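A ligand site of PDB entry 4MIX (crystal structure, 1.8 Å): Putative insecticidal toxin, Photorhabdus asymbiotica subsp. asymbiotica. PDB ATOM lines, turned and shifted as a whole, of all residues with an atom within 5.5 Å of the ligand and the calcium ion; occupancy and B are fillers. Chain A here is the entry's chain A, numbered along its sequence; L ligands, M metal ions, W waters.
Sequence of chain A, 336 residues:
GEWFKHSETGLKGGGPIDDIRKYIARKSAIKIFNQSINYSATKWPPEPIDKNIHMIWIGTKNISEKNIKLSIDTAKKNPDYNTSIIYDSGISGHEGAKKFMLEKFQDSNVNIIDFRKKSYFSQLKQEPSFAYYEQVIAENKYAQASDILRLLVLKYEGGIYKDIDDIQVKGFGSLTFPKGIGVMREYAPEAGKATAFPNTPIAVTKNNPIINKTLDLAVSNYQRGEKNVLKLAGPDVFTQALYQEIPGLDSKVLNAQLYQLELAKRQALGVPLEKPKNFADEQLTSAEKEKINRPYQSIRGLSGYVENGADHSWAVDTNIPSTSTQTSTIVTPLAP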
ATOM      1  N   ILE A  56       8.141  -0.020  -9.398  1.00  0.00           N
ATOM      2  CA  ILE A  56       9.525  -0.236  -9.865  1.00  0.00           C
ATOM      3  C   ILE A  56      10.514  -0.297  -8.701  1.00  0.00           C
ATOM      4  O   ILE A  56      10.569   0.617  -7.866  1.00  0.00           O
ATOM      5  CB  ILE A  56       9.968   0.842 -10.901  1.00  0.00           C
ATOM      6  CG1 ILE A  56       9.278   0.611 -12.250  1.00  0.00           C
ATOM      7  CG2 ILE A  56      11.489   0.828 -11.104  1.00  0.00           C
ATOM      8  CD1 ILE A  56       9.262   1.866 -13.108  1.00  0.00           C
ATOM      9  N   TRP A  57      11.271  -1.382  -8.659  1.00  0.00           N
ATOM     10  CA  TRP A  57      12.470  -1.421  -7.849  1.00  0.00           C
ATOM     11  C   TRP A  57      13.641  -2.069  -8.628  1.00  0.00           C
ATOM     12  O   TRP A  57      13.810  -3.308  -8.655  1.00  0.00           O
ATOM     13  CB  TRP A  57      12.244  -2.055  -6.484  1.00  0.00           C
ATOM     14  CG  TRP A  57      13.375  -1.786  -5.553  1.00  0.00           C
ATOM     15  CD1 TRP A  57      14.296  -2.679  -5.105  1.00  0.00           C
ATOM     16  CD2 TRP A  57      13.753  -0.510  -5.001  1.00  0.00           C
ATOM     17  NE1 TRP A  57      15.201  -2.060  -4.296  1.00  0.00           N
ATOM     18  CE2 TRP A  57      14.901  -0.722  -4.212  1.00  0.00           C
ATOM     19  CE3 TRP A  57      13.231   0.786  -5.096  1.00  0.00           C
ATOM     20  CZ2 TRP A  57      15.536   0.324  -3.502  1.00  0.00           C
ATOM     21  CZ3 TRP A  57      13.853   1.830  -4.393  1.00  0.00           C
ATOM     22  CH2 TRP A  57      15.009   1.586  -3.622  1.00  0.00           C
ATOM     23  N   ILE A  58      14.396  -1.220  -9.301  1.00  0.00           N
ATOM     24  CA  ILE A  58      15.537  -1.661 -10.103  1.00  0.00           C
ATOM     25  C   ILE A  58      16.818  -1.321  -9.366  1.00  0.00           C
ATOM     26  O   ILE A  58      16.833  -0.502  -8.430  1.00  0.00           O
ATOM     27  CB  ILE A  58      15.564  -1.043 -11.530  1.00  0.00           C
ATOM     28  CG1 ILE A  58      15.506   0.503 -11.448  1.00  0.00           C
ATOM     29  CG2 ILE A  58      14.399  -1.543 -12.384  1.00  0.00           C
ATOM     30  CD1 ILE A  58      15.670   1.223 -12.775  1.00  0.00           C
ATOM     31  N   GLY A  59      17.912  -1.957  -9.763  1.00  0.00           N
ATOM     32  CA  GLY A  59      19.222  -1.566  -9.245  1.00  0.00           C
ATOM     33  C   GLY A  59      19.821  -2.679  -8.431  1.00  0.00           C
ATOM     34  O   GLY A  59      19.605  -3.871  -8.717  1.00  0.00           O
ATOM     35  N   LYS A  61      20.509  -2.214  -4.705  1.00  0.00           N
ATOM     36  CA  LYS A  61      20.214  -2.048  -3.285  1.00  0.00           C
ATOM     37  C   LYS A  61      18.946  -2.831  -2.898  1.00  0.00           C
ATOM     38  O   LYS A  61      17.954  -2.814  -3.631  1.00  0.00           O
ATOM     39  CB  LYS A  61      20.049  -0.552  -2.961  1.00  0.00           C
ATOM     40  CG  LYS A  61      19.543  -0.235  -1.552  1.00  0.00           C
ATOM     41  CD  LYS A  61      18.973   1.183  -1.492  1.00  0.00           C
ATOM     42  CE  LYS A  61      18.961   1.707  -0.057  1.00  0.00           C
ATOM     43  NZ  LYS A  61      18.621   3.148   0.002  1.00  0.00           N
ATOM     44  N   TYR A 142      19.402   5.002 -10.858  1.00  0.00           N
ATOM     45  CA  TYR A 142      18.151   4.249 -10.862  1.00  0.00           C
ATOM     46  C   TYR A 142      16.892   5.088 -10.710  1.00  0.00           C
ATOM     47  O   TYR A 142      15.910   4.819 -11.380  1.00  0.00           O
ATOM     48  CB  TYR A 142      18.236   3.106  -9.820  1.00  0.00           C
ATOM     49  CG  TYR A 142      19.511   2.307 -10.004  1.00  0.00           C
ATOM     50  CD1 TYR A 142      19.859   1.781 -11.257  1.00  0.00           C
ATOM     51  CD2 TYR A 142      20.360   2.033  -8.922  1.00  0.00           C
ATOM     52  CE1 TYR A 142      21.040   1.079 -11.438  1.00  0.00           C
ATOM     53  CE2 TYR A 142      21.551   1.332  -9.106  1.00  0.00           C
ATOM     54  CZ  TYR A 142      21.873   0.843 -10.356  1.00  0.00           C
ATOM     55  OH  TYR A 142      23.031   0.148 -10.542  1.00  0.00           O
ATOM     56  N   ALA A 143      16.907   6.103  -9.836  1.00  0.00           N
ATOM     57  CA  ALA A 143      15.698   6.949  -9.690  1.00  0.00           C
ATOM     58  C   ALA A 143      15.392   7.674 -11.000  1.00  0.00           C
ATOM     59  O   ALA A 143      14.262   7.689 -11.479  1.00  0.00           O
ATOM     60  CB  ALA A 143      15.896   7.948  -8.553  1.00  0.00           C
ATOM     61  N   GLN A 144      16.423   8.234 -11.608  1.00  0.00           N
ATOM     62  CA  GLN A 144      16.262   8.931 -12.905  1.00  0.00           C
ATOM     63  C   GLN A 144      15.747   7.982 -13.994  1.00  0.00           C
ATOM     64  O   GLN A 144      14.815   8.330 -14.756  1.00  0.00           O
ATOM     65  CB  GLN A 144      17.589   9.555 -13.328  1.00  0.00           C
ATOM     66  CG  GLN A 144      17.532  10.284 -14.652  1.00  0.00           C
ATOM     67  CD  GLN A 144      18.878  10.880 -14.992  1.00  0.00           C
ATOM     68  OE1 GLN A 144      19.663  11.196 -14.099  1.00  0.00           O
ATOM     69  NE2 GLN A 144      19.156  11.044 -16.257  1.00  0.00           N
ATOM     70  N   SER A 146      13.906   5.309 -13.663  1.00  0.00           N
ATOM     71  CA  SER A 146      12.503   4.948 -13.417  1.00  0.00           C
ATOM     72  C   SER A 146      11.523   5.945 -14.043  1.00  0.00           C
ATOM     73  O   SER A 146      10.385   5.590 -14.281  1.00  0.00           O
ATOM     74  CB  SER A 146      12.193   4.795 -11.922  1.00  0.00           C
ATOM     75  OG  SER A 146      12.044   6.066 -11.270  1.00  0.00           O
ATOM     76  N   ASP A 147      11.954   7.196 -14.245  1.00  0.00           N
ATOM     77  CA  ASP A 147      11.128   8.154 -14.965  1.00  0.00           C
ATOM     78  C   ASP A 147      10.834   7.738 -16.396  1.00  0.00           C
ATOM     79  O   ASP A 147       9.747   8.020 -16.909  1.00  0.00           O
ATOM     80  CB  ASP A 147      11.760   9.549 -14.955  1.00  0.00           C
ATOM     81  CG  ASP A 147      11.660  10.216 -13.579  1.00  0.00           C
ATOM     82  OD1 ASP A 147      11.027   9.635 -12.668  1.00  0.00           O
ATOM     83  OD2 ASP A 147      12.251  11.319 -13.405  1.00  0.00           O
ATOM     84  N   ARG A 150       8.853   3.848 -16.224  1.00  0.00           N
ATOM     85  CA  ARG A 150       7.400   3.853 -15.913  1.00  0.00           C
ATOM     86  C   ARG A 150       6.573   4.203 -17.162  1.00  0.00           C
ATOM     87  O   ARG A 150       5.484   3.658 -17.344  1.00  0.00           O
ATOM     88  CB  ARG A 150       7.081   4.772 -14.731  1.00  0.00           C
ATOM     89  CG  ARG A 150       7.117   6.262 -15.092  1.00  0.00           C
ATOM     90  CD  ARG A 150       6.944   7.146 -13.864  1.00  0.00           C
ATOM     91  NE  ARG A 150       8.145   7.097 -13.053  1.00  0.00           N
ATOM     92  CZ  ARG A 150       8.289   7.629 -11.847  1.00  0.00           C
ATOM     93  NH1 ARG A 150       7.292   8.327 -11.299  1.00  0.00           N
ATOM     94  NH2 ARG A 150       9.435   7.503 -11.197  1.00  0.00           N
ATOM     95  N   TYR A 161       0.554   3.074 -12.554  1.00  0.00           N
ATOM     96  CA  TYR A 161       1.889   3.141 -11.972  1.00  0.00           C
ATOM     97  C   TYR A 161       1.812   3.802 -10.591  1.00  0.00           C
ATOM     98  O   TYR A 161       1.163   4.835 -10.415  1.00  0.00           O
ATOM     99  CB  TYR A 161       2.889   3.920 -12.858  1.00  0.00           C
ATOM    100  CG  TYR A 161       4.207   4.082 -12.137  1.00  0.00           C
ATOM    101  CD1 TYR A 161       5.083   3.003 -12.016  1.00  0.00           C
ATOM    102  CD2 TYR A 161       4.540   5.287 -11.518  1.00  0.00           C
ATOM    103  CE1 TYR A 161       6.279   3.123 -11.325  1.00  0.00           C
ATOM    104  CE2 TYR A 161       5.724   5.425 -10.826  1.00  0.00           C
ATOM    105  CZ  TYR A 161       6.582   4.341 -10.731  1.00  0.00           C
ATOM    106  OH  TYR A 161       7.745   4.466 -10.041  1.00  0.00           O
ATOM    107  N   ASP A 163       4.408   4.753  -7.013  1.00  0.00           N
ATOM    108  CA  ASP A 163       5.719   4.826  -6.339  1.00  0.00           C
ATOM    109  C   ASP A 163       5.836   3.809  -5.221  1.00  0.00           C
ATOM    110  O   ASP A 163       4.911   3.673  -4.406  1.00  0.00           O
ATOM    111  CB  ASP A 163       5.953   6.236  -5.764  1.00  0.00           C
ATOM    112  CG  ASP A 163       6.925   7.048  -6.594  1.00  0.00           C
ATOM    113  OD1 ASP A 163       6.832   6.998  -7.838  1.00  0.00           O
ATOM    114  OD2 ASP A 163       7.798   7.721  -5.995  1.00  0.00           O
ATOM    115  N   ILE A 164       6.973   3.116  -5.178  1.00  0.00           N
ATOM    116  CA  ILE A 164       7.213   2.051  -4.186  1.00  0.00           C
ATOM    117  C   ILE A 164       7.073   2.528  -2.736  1.00  0.00           C
ATOM    118  O   ILE A 164       6.715   1.750  -1.858  1.00  0.00           O
ATOM    119  CB  ILE A 164       8.594   1.362  -4.431  1.00  0.00           C
ATOM    120  CG1 ILE A 164       8.698   0.015  -3.691  1.00  0.00           C
ATOM    121  CG2 ILE A 164       9.773   2.261  -4.110  1.00  0.00           C
ATOM    122  CD1 ILE A 164       8.370  -1.151  -4.603  1.00  0.00           C
ATOM    123  N   ASP A 165       7.325   3.821  -2.498  1.00  0.00           N
ATOM    124  CA  ASP A 165       7.343   4.381  -1.152  1.00  0.00           C
ATOM    125  C   ASP A 165       6.095   5.178  -0.754  1.00  0.00           C
ATOM    126  O   ASP A 165       6.067   5.801   0.311  1.00  0.00           O
ATOM    127  CB  ASP A 165       8.613   5.214  -0.902  1.00  0.00           C
ATOM    128  CG  ASP A 165       8.867   6.229  -1.986  1.00  0.00           C
ATOM    129  OD1 ASP A 165       7.963   6.475  -2.793  1.00  0.00           O
ATOM    130  OD2 ASP A 165       9.990   6.771  -2.058  1.00  0.00           O
ATOM    131  N   ASP A 166       5.059   5.155  -1.605  1.00  0.00           N
ATOM    132  CA  ASP A 166       3.790   5.770  -1.267  1.00  0.00           C
ATOM    133  C   ASP A 166       2.878   4.850  -0.481  1.00  0.00           C
ATOM    134  O   ASP A 166       2.773   3.645  -0.757  1.00  0.00           O
ATOM    135  CB  ASP A 166       3.073   6.268  -2.520  1.00  0.00           C
ATOM    136  CG  ASP A 166       3.675   7.567  -3.057  1.00  0.00           C
ATOM    137  OD1 ASP A 166       4.761   7.984  -2.569  1.00  0.00           O
ATOM    138  OD2 ASP A 166       3.068   8.170  -3.969  1.00  0.00           O
ATOM    139  N   TYR A 187       0.305  20.125  -8.025  1.00  0.00           N
ATOM    140  CA  TYR A 187       0.934  20.491  -6.752  1.00  0.00           C
ATOM    141  C   TYR A 187       0.367  21.777  -6.143  1.00  0.00           C
ATOM    142  O   TYR A 187      -0.263  22.574  -6.835  1.00  0.00           O
ATOM    143  CB  TYR A 187       2.436  20.630  -6.931  1.00  0.00           C
ATOM    144  CG  TYR A 187       3.151  19.323  -7.191  1.00  0.00           C
ATOM    145  CD1 TYR A 187       3.334  18.397  -6.161  1.00  0.00           C
ATOM    146  CD2 TYR A 187       3.663  19.024  -8.445  1.00  0.00           C
ATOM    147  CE1 TYR A 187       3.996  17.187  -6.387  1.00  0.00           C
ATOM    148  CE2 TYR A 187       4.328  17.833  -8.686  1.00  0.00           C
ATOM    149  CZ  TYR A 187       4.492  16.915  -7.651  1.00  0.00           C
ATOM    150  OH  TYR A 187       5.159  15.736  -7.884  1.00  0.00           O
ATOM    151  N   ASN A 199       4.098  12.871 -11.680  1.00  0.00           N
ATOM    152  CA  ASN A 199       4.189  11.746 -12.590  1.00  0.00           C
ATOM    153  C   ASN A 199       4.033  10.425 -11.827  1.00  0.00           C
ATOM    154  O   ASN A 199       4.598   9.406 -12.223  1.00  0.00           O
ATOM    155  CB  ASN A 199       5.472  11.756 -13.454  1.00  0.00           C
ATOM    156  CG  ASN A 199       6.758  11.607 -12.642  1.00  0.00           C
ATOM    157  OD1 ASN A 199       6.811  11.890 -11.444  1.00  0.00           O
ATOM    158  ND2 ASN A 199       7.818  11.139 -13.309  1.00  0.00           N
ATOM    159  N   THR A 200       3.249  10.471 -10.746  1.00  0.00           N
ATOM    160  CA  THR A 200       2.886   9.300  -9.921  1.00  0.00           C
ATOM    161  C   THR A 200       1.803   9.732  -8.913  1.00  0.00           C
ATOM    162  O   THR A 200       1.846  10.852  -8.404  1.00  0.00           O
ATOM    163  CB  THR A 200       4.111   8.697  -9.189  1.00  0.00           C
ATOM    164  OG1 THR A 200       3.658   7.627  -8.342  1.00  0.00           O
ATOM    165  CG2 THR A 200       4.840   9.744  -8.319  1.00  0.00           C
ATOM    166  N   VAL A 229      17.538  17.013 -13.855  1.00  0.00           N
ATOM    167  CA  VAL A 229      16.956  15.652 -13.992  1.00  0.00           C
ATOM    168  C   VAL A 229      15.438  15.676 -14.066  1.00  0.00           C
ATOM    169  O   VAL A 229      14.835  14.877 -14.792  1.00  0.00           O
ATOM    170  CB  VAL A 229      17.452  14.646 -12.908  1.00  0.00           C
ATOM    171  CG1 VAL A 229      18.949  14.403 -13.036  1.00  0.00           C
ATOM    172  CG2 VAL A 229      17.102  15.097 -11.495  1.00  0.00           C
ATOM    173  N   LEU A 230      14.825  16.621 -13.358  1.00  0.00           N
ATOM    174  CA  LEU A 230      13.364  16.751 -13.382  1.00  0.00           C
ATOM    175  C   LEU A 230      12.818  17.243 -14.730  1.00  0.00           C
ATOM    176  O   LEU A 230      11.683  16.916 -15.079  1.00  0.00           O
ATOM    177  CB  LEU A 230      12.882  17.614 -12.204  1.00  0.00           C
ATOM    178  CG  LEU A 230      13.266  16.988 -10.849  1.00  0.00           C
ATOM    179  CD1 LEU A 230      12.958  17.898  -9.669  1.00  0.00           C
ATOM    180  CD2 LEU A 230      12.658  15.589 -10.654  1.00  0.00           C
ATOM    181  N   GLY A 234      10.565  14.162 -16.060  1.00  0.00           N
ATOM    182  CA  GLY A 234       9.882  14.367 -14.780  1.00  0.00           C
ATOM    183  C   GLY A 234       8.480  14.968 -14.854  1.00  0.00           C
ATOM    184  O   GLY A 234       7.885  15.017 -15.916  1.00  0.00           O
ATOM    185  N   PRO A 235       7.930  15.402 -13.704  1.00  0.00           N
ATOM    186  CA  PRO A 235       6.565  15.940 -13.653  1.00  0.00           C
ATOM    187  C   PRO A 235       6.360  17.137 -14.592  1.00  0.00           C
ATOM    188  O   PRO A 235       5.265  17.328 -15.098  1.00  0.00           O
ATOM    189  CB  PRO A 235       6.374  16.371 -12.180  1.00  0.00           C
ATOM    190  CG  PRO A 235       7.647  16.096 -11.482  1.00  0.00           C
ATOM    191  CD  PRO A 235       8.547  15.295 -12.365  1.00  0.00           C
HETATM  192  C1  LIG L   1      11.557  12.870  -7.423  1.00  0.00           C
HETATM  193  C2  LIG L   1      10.403  13.511  -8.182  1.00  0.00           C
HETATM  194  C3  LIG L   1       9.685  12.476  -9.047  1.00  0.00           C
HETATM  195  C4  LIG L   1      10.651  11.704  -9.945  1.00  0.00           C
HETATM  196  C5  LIG L   1      11.847  11.185  -9.143  1.00  0.00           C
HETATM  197  C6  LIG L   1      12.938  10.565 -10.028  1.00  0.00           C
HETATM  198  C7  LIG L   1       9.124  15.347  -7.271  1.00  0.00           C
HETATM  199  C8  LIG L   1       8.019  15.778  -6.330  1.00  0.00           C
HETATM  200  N1  LIG L   1       9.449  14.047  -7.231  1.00  0.00           N
HETATM  201  O1  LIG L   1      10.997  11.923  -6.509  1.00  0.00           O
HETATM  202  O2  LIG L   1       8.615  13.070  -9.794  1.00  0.00           O
HETATM  203  O3  LIG L   1       9.899  10.602 -10.450  1.00  0.00           O
HETATM  204  O4  LIG L   1      12.456  12.227  -8.351  1.00  0.00           O
HETATM  205  O5  LIG L   1      13.438  11.552 -10.951  1.00  0.00           O
HETATM  206  O6  LIG L   1       9.692  16.129  -8.023  1.00  0.00           O
HETATM  207  N2  LIG L   1      14.106   3.559  -7.641  1.00  0.00           N
HETATM  208  C9  LIG L   1      14.582   2.238  -7.889  1.00  0.00           C
HETATM  209  N3  LIG L   1      15.780   1.876  -7.419  1.00  0.00           N
HETATM  210  C10 LIG L   1      16.553   2.719  -6.710  1.00  0.00           C
HETATM  211  C11 LIG L   1      16.131   4.037  -6.458  1.00  0.00           C
HETATM  212  C12 LIG L   1      14.879   4.422  -6.925  1.00  0.00           C
HETATM  213  O7  LIG L   1      13.884   1.411  -8.559  1.00  0.00           O
HETATM  214  O8  LIG L   1      17.658   2.315  -6.311  1.00  0.00           O
HETATM  215  C13 LIG L   1      12.796   3.968  -8.179  1.00  0.00           C
HETATM  216  C14 LIG L   1      11.646   3.746  -7.207  1.00  0.00           C
HETATM  217  O9  LIG L   1      10.538   3.226  -7.958  1.00  0.00           O
HETATM  218  C15 LIG L   1      11.274   5.129  -6.716  1.00  0.00           C
HETATM  219  C16 LIG L   1      11.577   5.948  -7.975  1.00  0.00           C
HETATM  220  O10 LIG L   1      12.792   5.376  -8.494  1.00  0.00           O
HETATM  221  O11 LIG L   1       9.877   5.158  -6.353  1.00  0.00           O
HETATM  222  C17 LIG L   1      11.788   7.415  -7.677  1.00  0.00           C
HETATM  223  O12 LIG L   1      12.814   7.522  -6.699  1.00  0.00           O
HETATM  224  P1  LIG L   1      12.679   8.477  -5.431  1.00  0.00           P
HETATM  225  O13 LIG L   1      11.509   8.008  -4.636  1.00  0.00           O
HETATM  226  O14 LIG L   1      14.048   8.592  -4.824  1.00  0.00           O
HETATM  227  O15 LIG L   1      12.340   9.881  -6.159  1.00  0.00           O
HETATM  228  P2  LIG L   1      11.874  11.232  -5.380  1.00  0.00           P
HETATM  229  O16 LIG L   1      13.101  12.070  -5.129  1.00  0.00           O
HETATM  230  O17 LIG L   1      10.924  10.882  -4.260  1.00  0.00           O
HETATM  231 CA    CA M   1       9.351   8.749  -4.096  1.00  0.00          CA
HETATM  232  O   HOH W   1       7.109   8.805  -3.201  1.00  0.00           O
HETATM  233  O   HOH W   2      19.298   4.078  -5.231  1.00  0.00           O
HETATM  234  O   HOH W   3       7.530   2.339  -8.044  1.00  0.00           O
HETATM  235  O   HOH W   4       7.989  12.364  -5.723  1.00  0.00           O
HETATM  236  O   HOH W   5       6.015  13.712  -8.922  1.00  0.00           O
HETATM  237  O   HOH W   6       8.668   9.113  -8.694  1.00  0.00           O
HETATM  238  O   HOH W   7      19.949   0.318  -6.251  1.00  0.00           O
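Two residues have an atom within 4 Å of the calcium ion: Asp 163 and Asp 165.
The calcium ion is bound by an oxygen (O13) of the ligand (2.3 Å), water W1 (2.4 Å), an oxygen (O17) of the ligand (2.7 Å) and the side-chain carboxylate (OD2) of Asp 163 (2.7 Å).
The calcium ion has four donor atoms within binding distance.
Slightly farther from the calcium ion lies the side-chain carboxylate (OD2) of Asp 165 (2.9 Å).
Slightly farther from the calcium ion lies the side-chain carboxylate (OD1) of Asp 165 (3.0 Å).
The backbone carbonyl oxygen (O) of Ile 56 lies within hydrogen-bond range of an oxygen (O9) of the ligand.
O3 of the ligand lies within hydrogen-bond range of OD1 of Asp 147 (2.7 Å).
An oxygen (O2) of the ligand is in hydrogen-bond range of the side-chain amide oxygen (OD1) of Asn 199 (2.7 Å).
The backbone NH of Ile 58 is in hydrogen-bond range of an oxygen (O7) of the ligand (2.8 Å).
A nitrogen (N3) of the ligand sits at hydrogen-bond distance from the backbone carbonyl oxygen (O) of Ile 58 (2.8 Å).
OG of Ser 146 is in hydrogen-bond range of O10 of the ligand (3.0 Å).
The guanidinium group of Arg 150 lies within hydrogen-bond range of an oxygen (O3) of the ligand (3.2 Å).
Merely in contact with the ligand: Trp 57, Tyr 142, Ala 143, Tyr 161, Ile 164, Tyr 187, Leu 230 and Pro 235.
16 residues have an atom within 4 Å of the ligand: Ile 56, Trp 57, Ile 58, Tyr 142, Ala 143, Ser 146, Asp 147, Arg 150, Tyr 161, Asp 163, Ile 164, Asp 165, Tyr 187, Asn 199, Leu 230 and Pro 235.
Along chain A the residues within 4 Å of the ligand span positions 56 to 235.
OD1 of Asp 163 is in salt-bridge range of NH1 of Arg 150.
OD1 of Asp 163 is in hydrogen-bond range of OH of Tyr 161.
The backbone NH of Asp 163 is in hydrogen-bond range of the side-chain hydroxyl of Thr 200, at 3.3 Å.
OD1 of Asp 147 is in salt-bridge range of NH2 of Arg 150.
The backbone carbonyl oxygen (O) of Asn 199 lies within hydrogen-bond range of the guanidinium group (NH1) of Arg 150 (3.0 Å).
The guanidinium group (NE) of Arg 150 lies within hydrogen-bond range of the backbone carbonyl oxygen (O) of Ser 146 (3.0 Å).
The side-chain hydroxyl of Ser 146 lies within hydrogen-bond range of the backbone carbonyl oxygen of Ala 143 (2.8 Å).
The indole nitrogen (NE1) of Trp 57 lies within hydrogen-bond range of the backbone carbonyl oxygen (O) of Lys 61 (2.9 Å).
Water W1 lies within hydrogen-bond range of OD1 of Asp 165 (2.5 Å) and OD1 of Asp 166 (2.6 Å).
Water W6 lies within hydrogen-bond range of an oxygen (O3) of the ligand (2.6 Å), the side-chain carboxylate of Asp 163 (2.9 Å) and the guanidinium group of Arg 150 (3.0 Å).
Water W5 lies within hydrogen-bond range of OH of Tyr 187 (2.4 Å), O2 of the ligand (2.8 Å) and OD1 of Asn 199 (3.2 Å).
Water W7 bridges N of Lys 61 (3.0 Å) and O8 of the ligand (3.0 Å).
Water W3 lies within hydrogen-bond range of the backbone NH of Ile 56, the side-chain hydroxyl of Tyr 161, the backbone NH of Ile 164 and an oxygen (O9) of the ligand.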
